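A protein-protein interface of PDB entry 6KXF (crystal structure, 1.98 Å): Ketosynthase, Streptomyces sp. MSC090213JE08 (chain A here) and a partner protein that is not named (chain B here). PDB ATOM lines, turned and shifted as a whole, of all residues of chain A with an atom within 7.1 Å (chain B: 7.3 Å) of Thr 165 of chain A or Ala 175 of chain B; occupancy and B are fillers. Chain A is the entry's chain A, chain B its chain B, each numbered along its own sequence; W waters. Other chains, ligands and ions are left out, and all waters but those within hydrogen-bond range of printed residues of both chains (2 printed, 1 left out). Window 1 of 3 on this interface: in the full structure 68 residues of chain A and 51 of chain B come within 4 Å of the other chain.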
ATOM      1  N   ILE A 107      12.624 -12.015 -24.971  1.00  0.00           N
ATOM      2  CA  ILE A 107      12.430 -12.101 -23.502  1.00  0.00           C
ATOM      3  C   ILE A 107      13.559 -11.280 -22.881  1.00  0.00           C
ATOM      4  O   ILE A 107      14.714 -11.623 -23.082  1.00  0.00           O
ATOM      5  CB  ILE A 107      12.420 -13.559 -22.976  1.00  0.00           C
ATOM      6  CG1 ILE A 107      11.253 -14.360 -23.557  1.00  0.00           C
ATOM      7  CG2 ILE A 107      12.355 -13.526 -21.468  1.00  0.00           C
ATOM      8  CD1 ILE A 107      11.233 -15.833 -23.158  1.00  0.00           C
ATOM      9  N   THR A 108      13.229 -10.148 -22.246  1.00  0.00           N
ATOM     10  CA  THR A 108      14.260  -9.332 -21.648  1.00  0.00           C
ATOM     11  C   THR A 108      13.855  -8.982 -20.214  1.00  0.00           C
ATOM     12  O   THR A 108      12.797  -8.421 -19.983  1.00  0.00           O
ATOM     13  CB  THR A 108      14.723  -8.193 -22.570  1.00  0.00           C
ATOM     14  OG1 THR A 108      15.275  -7.075 -21.860  1.00  0.00           O
ATOM     15  CG2 THR A 108      13.674  -7.733 -23.524  1.00  0.00           C
ATOM     16  N   VAL A 109      14.746  -9.351 -19.292  1.00  0.00           N
ATOM     17  CA  VAL A 109      14.593  -9.194 -17.890  1.00  0.00           C
ATOM     18  C   VAL A 109      15.701  -8.290 -17.341  1.00  0.00           C
ATOM     19  O   VAL A 109      16.908  -8.511 -17.588  1.00  0.00           O
ATOM     20  CB  VAL A 109      14.645 -10.566 -17.192  1.00  0.00           C
ATOM     21  CG1 VAL A 109      14.444 -10.386 -15.690  1.00  0.00           C
ATOM     22  CG2 VAL A 109      13.653 -11.547 -17.799  1.00  0.00           C
ATOM     23  N   GLY A 110      15.296  -7.294 -16.555  1.00  0.00           N
ATOM     24  CA  GLY A 110      16.229  -6.368 -15.927  1.00  0.00           C
ATOM     25  C   GLY A 110      16.621  -6.852 -14.559  1.00  0.00           C
ATOM     26  O   GLY A 110      15.801  -7.440 -13.862  1.00  0.00           O
ATOM     27  N   THR A 111      17.877  -6.648 -14.178  1.00  0.00           N
ATOM     28  CA  THR A 111      18.279  -6.984 -12.797  1.00  0.00           C
ATOM     29  C   THR A 111      19.392  -6.051 -12.358  1.00  0.00           C
ATOM     30  O   THR A 111      20.108  -5.549 -13.192  1.00  0.00           O
ATOM     31  CB  THR A 111      18.691  -8.461 -12.647  1.00  0.00           C
ATOM     32  OG1 THR A 111      18.630  -8.883 -11.282  1.00  0.00           O
ATOM     33  CG2 THR A 111      20.109  -8.731 -13.100  1.00  0.00           C
ATOM     34  N   ASN A 144      25.038 -16.446 -12.787  1.00  0.00           N
ATOM     35  CA  ASN A 144      25.294 -15.482 -13.886  1.00  0.00           C
ATOM     36  C   ASN A 144      23.964 -14.928 -14.410  1.00  0.00           C
ATOM     37  O   ASN A 144      23.035 -15.691 -14.753  1.00  0.00           O
ATOM     38  CB  ASN A 144      26.104 -16.118 -15.008  1.00  0.00           C
ATOM     39  CG  ASN A 144      27.507 -16.471 -14.551  1.00  0.00           C
ATOM     40  OD1 ASN A 144      28.113 -15.791 -13.713  1.00  0.00           O
ATOM     41  ND2 ASN A 144      28.043 -17.523 -15.122  1.00  0.00           N
ATOM     42  N   ALA A 145      23.892 -13.592 -14.501  1.00  0.00           N
ATOM     43  CA  ALA A 145      22.643 -12.878 -14.699  1.00  0.00           C
ATOM     44  C   ALA A 145      21.957 -13.274 -16.006  1.00  0.00           C
ATOM     45  O   ALA A 145      20.737 -13.113 -16.106  1.00  0.00           O
ATOM     46  CB  ALA A 145      22.874 -11.387 -14.627  1.00  0.00           C
ATOM     47  N   GLY A 146      22.707 -13.752 -17.020  1.00  0.00           N
ATOM     48  CA  GLY A 146      22.059 -14.117 -18.328  1.00  0.00           C
ATOM     49  C   GLY A 146      20.991 -15.208 -18.170  1.00  0.00           C
ATOM     50  O   GLY A 146      20.016 -15.335 -18.981  1.00  0.00           O
ATOM     51  N   ARG A 147      21.161 -16.022 -17.129  1.00  0.00           N
ATOM     52  CA  ARG A 147      20.258 -17.142 -16.763  1.00  0.00           C
ATOM     53  C   ARG A 147      18.834 -16.648 -16.432  1.00  0.00           C
ATOM     54  O   ARG A 147      17.864 -17.360 -16.671  1.00  0.00           O
ATOM     55  CB  ARG A 147      20.879 -17.905 -15.586  1.00  0.00           C
ATOM     56  CG  ARG A 147      20.101 -19.140 -15.148  1.00  0.00           C
ATOM     57  CD  ARG A 147      20.903 -19.974 -14.159  1.00  0.00           C
ATOM     58  NE  ARG A 147      22.006 -20.647 -14.837  1.00  0.00           N
ATOM     59  CZ  ARG A 147      22.047 -21.958 -15.050  1.00  0.00           C
ATOM     60  NH1 ARG A 147      21.210 -22.766 -14.407  1.00  0.00           N
ATOM     61  NH2 ARG A 147      22.947 -22.455 -15.872  1.00  0.00           N
ATOM     62  N   LEU A 148      18.695 -15.407 -15.934  1.00  0.00           N
ATOM     63  CA  LEU A 148      17.395 -14.886 -15.520  1.00  0.00           C
ATOM     64  C   LEU A 148      16.447 -14.815 -16.710  1.00  0.00           C
ATOM     65  O   LEU A 148      15.269 -14.966 -16.497  1.00  0.00           O
ATOM     66  CB  LEU A 148      17.486 -13.505 -14.865  1.00  0.00           C
ATOM     67  CG  LEU A 148      18.327 -13.419 -13.585  1.00  0.00           C
ATOM     68  CD1 LEU A 148      18.398 -11.974 -13.101  1.00  0.00           C
ATOM     69  CD2 LEU A 148      17.791 -14.321 -12.491  1.00  0.00           C
ATOM     70  N   SER A 149      16.958 -14.578 -17.933  1.00  0.00           N
ATOM     71  CA  SER A 149      16.079 -14.518 -19.089  1.00  0.00           C
ATOM     72  C   SER A 149      16.006 -15.880 -19.828  1.00  0.00           C
ATOM     73  O   SER A 149      14.939 -16.266 -20.303  1.00  0.00           O
ATOM     74  CB  SER A 149      16.499 -13.363 -20.003  1.00  0.00           C
ATOM     75  OG  SER A 149      17.887 -13.469 -20.344  1.00  0.00           O
ATOM     76  N   THR A 150      17.111 -16.639 -19.909  1.00  0.00           N
ATOM     77  CA  THR A 150      17.083 -17.933 -20.633  1.00  0.00           C
ATOM     78  C   THR A 150      16.159 -18.932 -19.908  1.00  0.00           C
ATOM     79  O   THR A 150      15.487 -19.711 -20.552  1.00  0.00           O
ATOM     80  CB  THR A 150      18.483 -18.512 -20.857  1.00  0.00           C
ATOM     81  OG1 THR A 150      19.107 -18.718 -19.594  1.00  0.00           O
ATOM     82  CG2 THR A 150      19.369 -17.626 -21.686  1.00  0.00           C
ATOM     83  N   ALA A 163      16.995 -13.925 -25.626  1.00  0.00           N
ATOM     84  CA  ALA A 163      16.867 -13.857 -24.198  1.00  0.00           C
ATOM     85  C   ALA A 163      18.002 -13.002 -23.653  1.00  0.00           C
ATOM     86  O   ALA A 163      19.167 -13.482 -23.499  1.00  0.00           O
ATOM     87  CB  ALA A 163      16.871 -15.239 -23.587  1.00  0.00           C
ATOM     88  N   THR A 164      17.663 -11.737 -23.378  1.00  0.00           N
ATOM     89  CA  THR A 164      18.629 -10.729 -22.902  1.00  0.00           C
ATOM     90  C   THR A 164      18.294 -10.295 -21.472  1.00  0.00           C
ATOM     91  O   THR A 164      17.155  -9.819 -21.180  1.00  0.00           O
ATOM     92  CB  THR A 164      18.652  -9.503 -23.827  1.00  0.00           C
ATOM     93  OG1 THR A 164      18.800  -9.950 -25.175  1.00  0.00           O
ATOM     94  CG2 THR A 164      19.739  -8.526 -23.449  1.00  0.00           C
ATOM     95  N   THR A 165      19.283 -10.411 -20.588  1.00  0.00           N
ATOM     96  CA  THR A 165      19.219  -9.833 -19.283  1.00  0.00           C
ATOM     97  C   THR A 165      19.910  -8.467 -19.316  1.00  0.00           C
ATOM     98  O   THR A 165      21.125  -8.361 -19.614  1.00  0.00           O
ATOM     99  CB  THR A 165      19.862 -10.729 -18.227  1.00  0.00           C
ATOM    100  OG1 THR A 165      19.157 -11.973 -18.256  1.00  0.00           O
ATOM    101  CG2 THR A 165      19.811 -10.098 -16.860  1.00  0.00           C
ATOM    102  N   VAL A 166      19.137  -7.409 -19.057  1.00  0.00           N
ATOM    103  CA  VAL A 166      19.640  -6.041 -19.054  1.00  0.00           C
ATOM    104  C   VAL A 166      20.030  -5.688 -17.627  1.00  0.00           C
ATOM    105  O   VAL A 166      19.159  -5.661 -16.731  1.00  0.00           O
ATOM    106  CB  VAL A 166      18.603  -5.034 -19.577  1.00  0.00           C
ATOM    107  CG1 VAL A 166      19.143  -3.598 -19.497  1.00  0.00           C
ATOM    108  CG2 VAL A 166      18.181  -5.362 -21.000  1.00  0.00           C
ATOM    109  N   THR A 167      21.307  -5.339 -17.455  1.00  0.00           N
ATOM    110  CA  THR A 167      21.938  -5.124 -16.185  1.00  0.00           C
ATOM    111  C   THR A 167      22.263  -3.634 -16.033  1.00  0.00           C
ATOM    112  O   THR A 167      23.441  -3.246 -15.836  1.00  0.00           O
ATOM    113  CB  THR A 167      23.164  -6.036 -16.009  1.00  0.00           C
ATOM    114  OG1 THR A 167      24.193  -5.712 -16.940  1.00  0.00           O
ATOM    115  CG2 THR A 167      22.830  -7.498 -16.204  1.00  0.00           C
ATOM    116  N   THR A 168      21.214  -2.804 -16.156  1.00  0.00           N
ATOM    117  CA  THR A 168      21.290  -1.341 -15.905  1.00  0.00           C
ATOM    118  C   THR A 168      20.629  -1.021 -14.560  1.00  0.00           C
ATOM    119  O   THR A 168      20.070   0.051 -14.378  1.00  0.00           O
ATOM    120  CB  THR A 168      20.652  -0.540 -17.035  1.00  0.00           C
ATOM    121  OG1 THR A 168      19.279  -0.927 -17.191  1.00  0.00           O
ATOM    122  CG2 THR A 168      21.386  -0.708 -18.344  1.00  0.00           C
ATOM    123  N   SER A 176      14.158  -2.703 -20.336  1.00  0.00           N
ATOM    124  CA  SER A 176      13.703  -3.986 -20.913  1.00  0.00           C
ATOM    125  C   SER A 176      12.375  -3.801 -21.638  1.00  0.00           C
ATOM    126  O   SER A 176      12.164  -4.333 -22.766  1.00  0.00           O
ATOM    127  CB  SER A 176      13.586  -5.073 -19.879  1.00  0.00           C
ATOM    128  OG  SER A 176      14.834  -5.376 -19.292  1.00  0.00           O
ATOM    129  N   LEU B 118      27.648  -2.555 -23.641  1.00  0.00           N
ATOM    130  CA  LEU B 118      28.662  -3.522 -23.240  1.00  0.00           C
ATOM    131  C   LEU B 118      27.991  -4.834 -22.768  1.00  0.00           C
ATOM    132  O   LEU B 118      26.973  -4.807 -22.035  1.00  0.00           O
ATOM    133  CB  LEU B 118      29.465  -2.885 -22.118  1.00  0.00           C
ATOM    134  CG  LEU B 118      30.795  -3.547 -21.798  1.00  0.00           C
ATOM    135  CD1 LEU B 118      31.756  -3.413 -22.978  1.00  0.00           C
ATOM    136  CD2 LEU B 118      31.369  -2.923 -20.532  1.00  0.00           C
ATOM    137  N   GLY B 119      28.500  -5.972 -23.260  1.00  0.00           N
ATOM    138  CA  GLY B 119      28.168  -7.297 -22.731  1.00  0.00           C
ATOM    139  C   GLY B 119      29.146  -7.755 -21.666  1.00  0.00           C
ATOM    140  O   GLY B 119      30.381  -7.516 -21.767  1.00  0.00           O
ATOM    141  N   ILE B 120      28.582  -8.417 -20.643  1.00  0.00           N
ATOM    142  CA  ILE B 120      29.275  -8.958 -19.472  1.00  0.00           C
ATOM    143  C   ILE B 120      28.734 -10.365 -19.149  1.00  0.00           C
ATOM    144  O   ILE B 120      27.735 -10.841 -19.758  1.00  0.00           O
ATOM    145  CB  ILE B 120      29.079  -8.060 -18.250  1.00  0.00           C
ATOM    146  CG1 ILE B 120      27.596  -8.018 -17.837  1.00  0.00           C
ATOM    147  CG2 ILE B 120      29.685  -6.688 -18.468  1.00  0.00           C
ATOM    148  CD1 ILE B 120      27.360  -7.349 -16.540  1.00  0.00           C
ATOM    149  N   THR B 121      29.354 -10.992 -18.150  1.00  0.00           N
ATOM    150  CA  THR B 121      28.870 -12.244 -17.624  1.00  0.00           C
ATOM    151  C   THR B 121      28.115 -11.949 -16.329  1.00  0.00           C
ATOM    152  O   THR B 121      26.884 -12.183 -16.256  1.00  0.00           O
ATOM    153  CB  THR B 121      29.976 -13.284 -17.405  1.00  0.00           C
ATOM    154  OG1 THR B 121      30.622 -13.598 -18.643  1.00  0.00           O
ATOM    155  CG2 THR B 121      29.409 -14.555 -16.795  1.00  0.00           C
ATOM    156  N   MET B 122      28.869 -11.489 -15.318  1.00  0.00           N
ATOM    157  CA  MET B 122      28.338 -11.125 -14.014  1.00  0.00           C
ATOM    158  C   MET B 122      29.199 -10.026 -13.376  1.00  0.00           C
ATOM    159  O   MET B 122      29.241  -9.872 -12.149  1.00  0.00           O
ATOM    160  CB  MET B 122      28.250 -12.341 -13.081  1.00  0.00           C
ATOM    161  CG  MET B 122      27.383 -12.114 -11.851  1.00  0.00           C
ATOM    162  SD  MET B 122      25.713 -11.500 -12.285  1.00  0.00           S
ATOM    163  CE  MET B 122      24.915 -11.508 -10.681  1.00  0.00           C
ATOM    164  N   GLY B 123      29.810  -9.196 -14.223  1.00  0.00           N
ATOM    165  CA  GLY B 123      30.531  -8.012 -13.751  1.00  0.00           C
ATOM    166  C   GLY B 123      31.770  -8.404 -12.966  1.00  0.00           C
ATOM    167  O   GLY B 123      32.420  -9.423 -13.271  1.00  0.00           O
ATOM    168  N   LEU B 154      27.004  -3.679 -12.015  1.00  0.00           N
ATOM    169  CA  LEU B 154      27.143  -4.384 -13.254  1.00  0.00           C
ATOM    170  C   LEU B 154      27.250  -3.375 -14.393  1.00  0.00           C
ATOM    171  O   LEU B 154      27.964  -3.641 -15.383  1.00  0.00           O
ATOM    172  CB  LEU B 154      25.949  -5.337 -13.448  1.00  0.00           C
ATOM    173  CG  LEU B 154      25.785  -6.433 -12.396  1.00  0.00           C
ATOM    174  CD1 LEU B 154      24.586  -7.334 -12.728  1.00  0.00           C
ATOM    175  CD2 LEU B 154      27.052  -7.265 -12.262  1.00  0.00           C
ATOM    176  N   THR B 172      23.878   1.222 -21.990  1.00  0.00           N
ATOM    177  CA  THR B 172      23.247  -0.059 -21.653  1.00  0.00           C
ATOM    178  C   THR B 172      24.337  -1.107 -21.377  1.00  0.00           C
ATOM    179  O   THR B 172      25.331  -1.160 -22.071  1.00  0.00           O
ATOM    180  CB  THR B 172      22.320  -0.550 -22.775  1.00  0.00           C
ATOM    181  OG1 THR B 172      21.341   0.441 -23.139  1.00  0.00           O
ATOM    182  CG2 THR B 172      21.633  -1.849 -22.394  1.00  0.00           C
ATOM    183  N   THR B 173      24.123  -1.939 -20.355  1.00  0.00           N
ATOM    184  CA  THR B 173      24.870  -3.146 -20.141  1.00  0.00           C
ATOM    185  C   THR B 173      23.907  -4.339 -20.276  1.00  0.00           C
ATOM    186  O   THR B 173      22.734  -4.299 -19.773  1.00  0.00           O
ATOM    187  CB  THR B 173      25.607  -3.077 -18.798  1.00  0.00           C
ATOM    188  OG1 THR B 173      26.358  -1.865 -18.700  1.00  0.00           O
ATOM    189  CG2 THR B 173      26.570  -4.222 -18.584  1.00  0.00           C
ATOM    190  N   VAL B 174      24.376  -5.385 -20.966  1.00  0.00           N
ATOM    191  CA  VAL B 174      23.633  -6.660 -21.078  1.00  0.00           C
ATOM    192  C   VAL B 174      24.507  -7.831 -20.593  1.00  0.00           C
ATOM    193  O   VAL B 174      25.708  -7.830 -20.794  1.00  0.00           O
ATOM    194  CB  VAL B 174      23.101  -6.884 -22.503  1.00  0.00           C
ATOM    195  CG1 VAL B 174      22.187  -5.743 -22.928  1.00  0.00           C
ATOM    196  CG2 VAL B 174      24.180  -7.102 -23.550  1.00  0.00           C
ATOM    197  N   ALA B 175      23.877  -8.852 -19.989  1.00  0.00           N
ATOM    198  CA  ALA B 175      24.599 -10.086 -19.587  1.00  0.00           C
ATOM    199  C   ALA B 175      24.601 -11.093 -20.749  1.00  0.00           C
ATOM    200  O   ALA B 175      24.340 -10.720 -21.888  1.00  0.00           O
ATOM    201  CB  ALA B 175      23.989 -10.670 -18.338  1.00  0.00           C
ATOM    202  N   GLY B 176      24.831 -12.376 -20.442  1.00  0.00           N
ATOM    203  CA  GLY B 176      24.757 -13.440 -21.426  1.00  0.00           C
ATOM    204  C   GLY B 176      26.062 -14.210 -21.620  1.00  0.00           C
ATOM    205  O   GLY B 176      26.101 -15.148 -22.418  1.00  0.00           O
ATOM    206  N   GLY B 177      27.121 -13.804 -20.922  1.00  0.00           N
ATOM    207  CA  GLY B 177      28.418 -14.473 -20.987  1.00  0.00           C
ATOM    208  C   GLY B 177      28.937 -14.503 -22.417  1.00  0.00           C
ATOM    209  O   GLY B 177      29.086 -13.474 -23.068  1.00  0.00           O
ATOM    210  N   ARG B 178      29.082 -15.707 -22.968  1.00  0.00           N
ATOM    211  CA  ARG B 178      29.802 -15.879 -24.206  1.00  0.00           C
ATOM    212  C   ARG B 178      28.992 -15.333 -25.380  1.00  0.00           C
ATOM    213  O   ARG B 178      29.581 -14.982 -26.382  1.00  0.00           O
ATOM    214  CB  ARG B 178      30.113 -17.357 -24.437  1.00  0.00           C
ATOM    215  CG  ARG B 178      31.113 -17.963 -23.466  1.00  0.00           C
ATOM    216  CD  ARG B 178      32.016 -18.914 -24.257  1.00  0.00           C
ATOM    217  NE  ARG B 178      32.666 -20.035 -23.588  1.00  0.00           N
ATOM    218  CZ  ARG B 178      32.456 -20.449 -22.338  1.00  0.00           C
ATOM    219  NH1 ARG B 178      32.473 -21.749 -22.075  1.00  0.00           N
ATOM    220  NH2 ARG B 178      32.259 -19.582 -21.355  1.00  0.00           N
ATOM    221  N   VAL B 179      27.650 -15.290 -25.277  1.00  0.00           N
ATOM    222  CA  VAL B 179      26.864 -14.710 -26.369  1.00  0.00           C
ATOM    223  C   VAL B 179      26.692 -13.188 -26.192  1.00  0.00           C
ATOM    224  O   VAL B 179      26.088 -12.570 -27.059  1.00  0.00           O
ATOM    225  CB  VAL B 179      25.482 -15.372 -26.545  1.00  0.00           C
ATOM    226  CG1 VAL B 179      25.605 -16.842 -26.950  1.00  0.00           C
ATOM    227  CG2 VAL B 179      24.599 -15.207 -25.311  1.00  0.00           C
ATOM    228  N   SER B 180      27.181 -12.608 -25.099  1.00  0.00           N
ATOM    229  CA  SER B 180      26.807 -11.210 -24.748  1.00  0.00           C
ATOM    230  C   SER B 180      27.270 -10.193 -25.817  1.00  0.00           C
ATOM    231  O   SER B 180      26.589  -9.160 -26.076  1.00  0.00           O
ATOM    232  CB  SER B 180      27.318 -10.876 -23.379  1.00  0.00           C
ATOM    233  OG  SER B 180      28.720 -10.740 -23.385  1.00  0.00           O
ATOM    234  N   GLY B 181      28.433 -10.435 -26.458  1.00  0.00           N
ATOM    235  CA  GLY B 181      28.881  -9.503 -27.512  1.00  0.00           C
ATOM    236  C   GLY B 181      27.876  -9.442 -28.628  1.00  0.00           C
ATOM    237  O   GLY B 181      27.706  -8.415 -29.257  1.00  0.00           O
ATOM    238  N   LEU B 183      24.531 -10.316 -28.324  1.00  0.00           N
ATOM    239  CA  LEU B 183      23.311  -9.683 -27.733  1.00  0.00           C
ATOM    240  C   LEU B 183      23.451  -8.160 -27.790  1.00  0.00           C
ATOM    241  O   LEU B 183      22.512  -7.463 -28.200  1.00  0.00           O
ATOM    242  CB  LEU B 183      23.149 -10.160 -26.289  1.00  0.00           C
ATOM    243  CG  LEU B 183      22.710 -11.618 -26.139  1.00  0.00           C
ATOM    244  CD1 LEU B 183      22.354 -11.961 -24.694  1.00  0.00           C
ATOM    245  CD2 LEU B 183      21.540 -11.927 -27.057  1.00  0.00           C
ATOM    246  N   ALA B 184      24.651  -7.684 -27.442  1.00  0.00           N
ATOM    247  CA  ALA B 184      25.011  -6.258 -27.489  1.00  0.00           C
ATOM    248  C   ALA B 184      24.923  -5.713 -28.923  1.00  0.00           C
ATOM    249  O   ALA B 184      24.319  -4.663 -29.161  1.00  0.00           O
ATOM    250  CB  ALA B 184      26.382  -6.078 -26.888  1.00  0.00           C
ATOM    251  N   ALA B 330      32.796 -13.321 -21.390  1.00  0.00           N
ATOM    252  CA  ALA B 330      31.951 -12.405 -22.126  1.00  0.00           C
ATOM    253  C   ALA B 330      32.703 -11.786 -23.301  1.00  0.00           C
ATOM    254  O   ALA B 330      32.071 -11.361 -24.281  1.00  0.00           O
ATOM    255  CB  ALA B 330      31.412 -11.343 -21.190  1.00  0.00           C
HETATM  256  O   HOH W   1      21.679 -11.661 -21.276  1.00  0.00           O
HETATM  257  O   HOH W   2      19.986  -8.381 -27.167  1.00  0.00           O
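The backbone NH (N) of Ala 145 of chain A lies within hydrogen-bond range of the side-chain sulfur (SD) of Met 122 of chain B (3.6 Å).
The backbone NH (N) of Ala 175 of chain B is in hydrogen-bond range of the backbone carbonyl oxygen (O) of Thr 165 of chain A (2.8 Å).
The backbone NH (N) of Thr 167 of chain A lies within hydrogen-bond range of the backbone carbonyl oxygen (O) of Thr 173 of chain B (2.9 Å).
The backbone carbonyl oxygen (O) of Val 109 of chain A lies within hydrogen-bond range of the backbone NH (N) of Val 166 of chain A (2.9 Å).
The backbone carbonyl oxygen (O) of Val 166 of chain A sits at hydrogen-bond distance from the backbone NH (N) of Thr 111 of chain A (3.0 Å).
The side-chain hydroxyl (OG) of Ser 149 of chain A lies close to the backbone carbonyl oxygen (O) of Ala 163 of chain A (3.4 Å).
The side-chain hydroxyl (OG) of Ser 149 of chain A lies within hydrogen-bond range of the side-chain hydroxyl (OG1) of Thr 165 of chain A, 2.9 Å away.
N of Ile 120 of chain B sits at hydrogen-bond distance from O of Val 174 of chain B (2.9 Å).
The backbone carbonyl oxygen (O) of Ile 120 of chain B is in hydrogen-bond range of the backbone NH (N) of Gly 177 of chain B (3.2 Å).
Among the printed residues, merely in contact across the chains: Thr 165 of chain A with Val 174 of chain B (3.4 Å), Asn 144 of chain A with Met 122 of chain B (3.5 Å), Asn 144 of chain A with Thr 121 of chain B (3.5 Å), Thr 167 of chain A with Ile 120 of chain B (3.6 Å), Gly 146 of chain A with Ala 175 of chain B (3.6 Å), Thr 168 of chain A with Thr 173 of chain B (3.6 Å), Val 166 of chain A with Thr 173 of chain B (3.6 Å), Ala 163 of chain A with Leu 183 of chain B (3.7 Å), Thr 164 of chain A with Val 174 of chain B (3.7 Å), Ala 145 of chain A with Thr 121 of chain B (3.7 Å), Thr 167 of chain A with Leu 154 of chain B (3.8 Å), Thr 168 of chain A with Thr 172 of chain B (3.9 Å), Thr 164 of chain A with Leu 183 of chain B (3.9 Å), Gly 146 of chain A with Gly 176 of chain B (3.9 Å), Ala 145 of chain A with Ala 175 of chain B (3.9 Å) and Thr 167 of chain A with Ala 175 of chain B (3.99 Å).
Of the printed residues of chain B, Asn 144 of chain A touches Thr 121 (3.5 Å) and Met 122 (3.5 Å).
Ser 149 of chain A touches none of the printed residues of chain B.
Thr 165 of chain A touches two residues of chain B.
Printed residues of chain A within 4 Å of Thr 172 of chain B: Thr 168.
Of the printed residues of chain A, Ala 175 of chain B touches Ala 145 (3.9 Å), Gly 146 (3.6 Å), Thr 165 (2.8 Å) and Thr 167 (3.99 Å).
The nearest printed residue of chain A that does not touch Ala 175 of chain B is Val 166 of chain A (5.0 Å).
Printed residues of chain B that touch a printed residue of chain A: Ile 120, Thr 121, Met 122, Leu 154, Thr 172, Thr 173, Val 174, Ala 175, Gly 176 and Leu 183.
Of the 19 printed residues of chain A, 9 touch a printed residue of chain B.
Hydrophobic or aromatic side chains of chain A within 4 Å of the printed part of chain B: Ala 145 and Val 166.
Among the printed residues, no Asp or Glu carboxylate lies within 4 Å of a Lys or Arg side-chain nitrogen of the other chain.
Water W1 lies within hydrogen-bond range of the backbone NH of Thr 165 of chain A, the backbone carbonyl oxygen of Ala 175 of chain B and the backbone NH of Gly 176 of chain B.
Water W2 bridges OG1 of Thr 164 of chain A (2.8 Å) and O of Leu 183 of chain B (2.9 Å).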
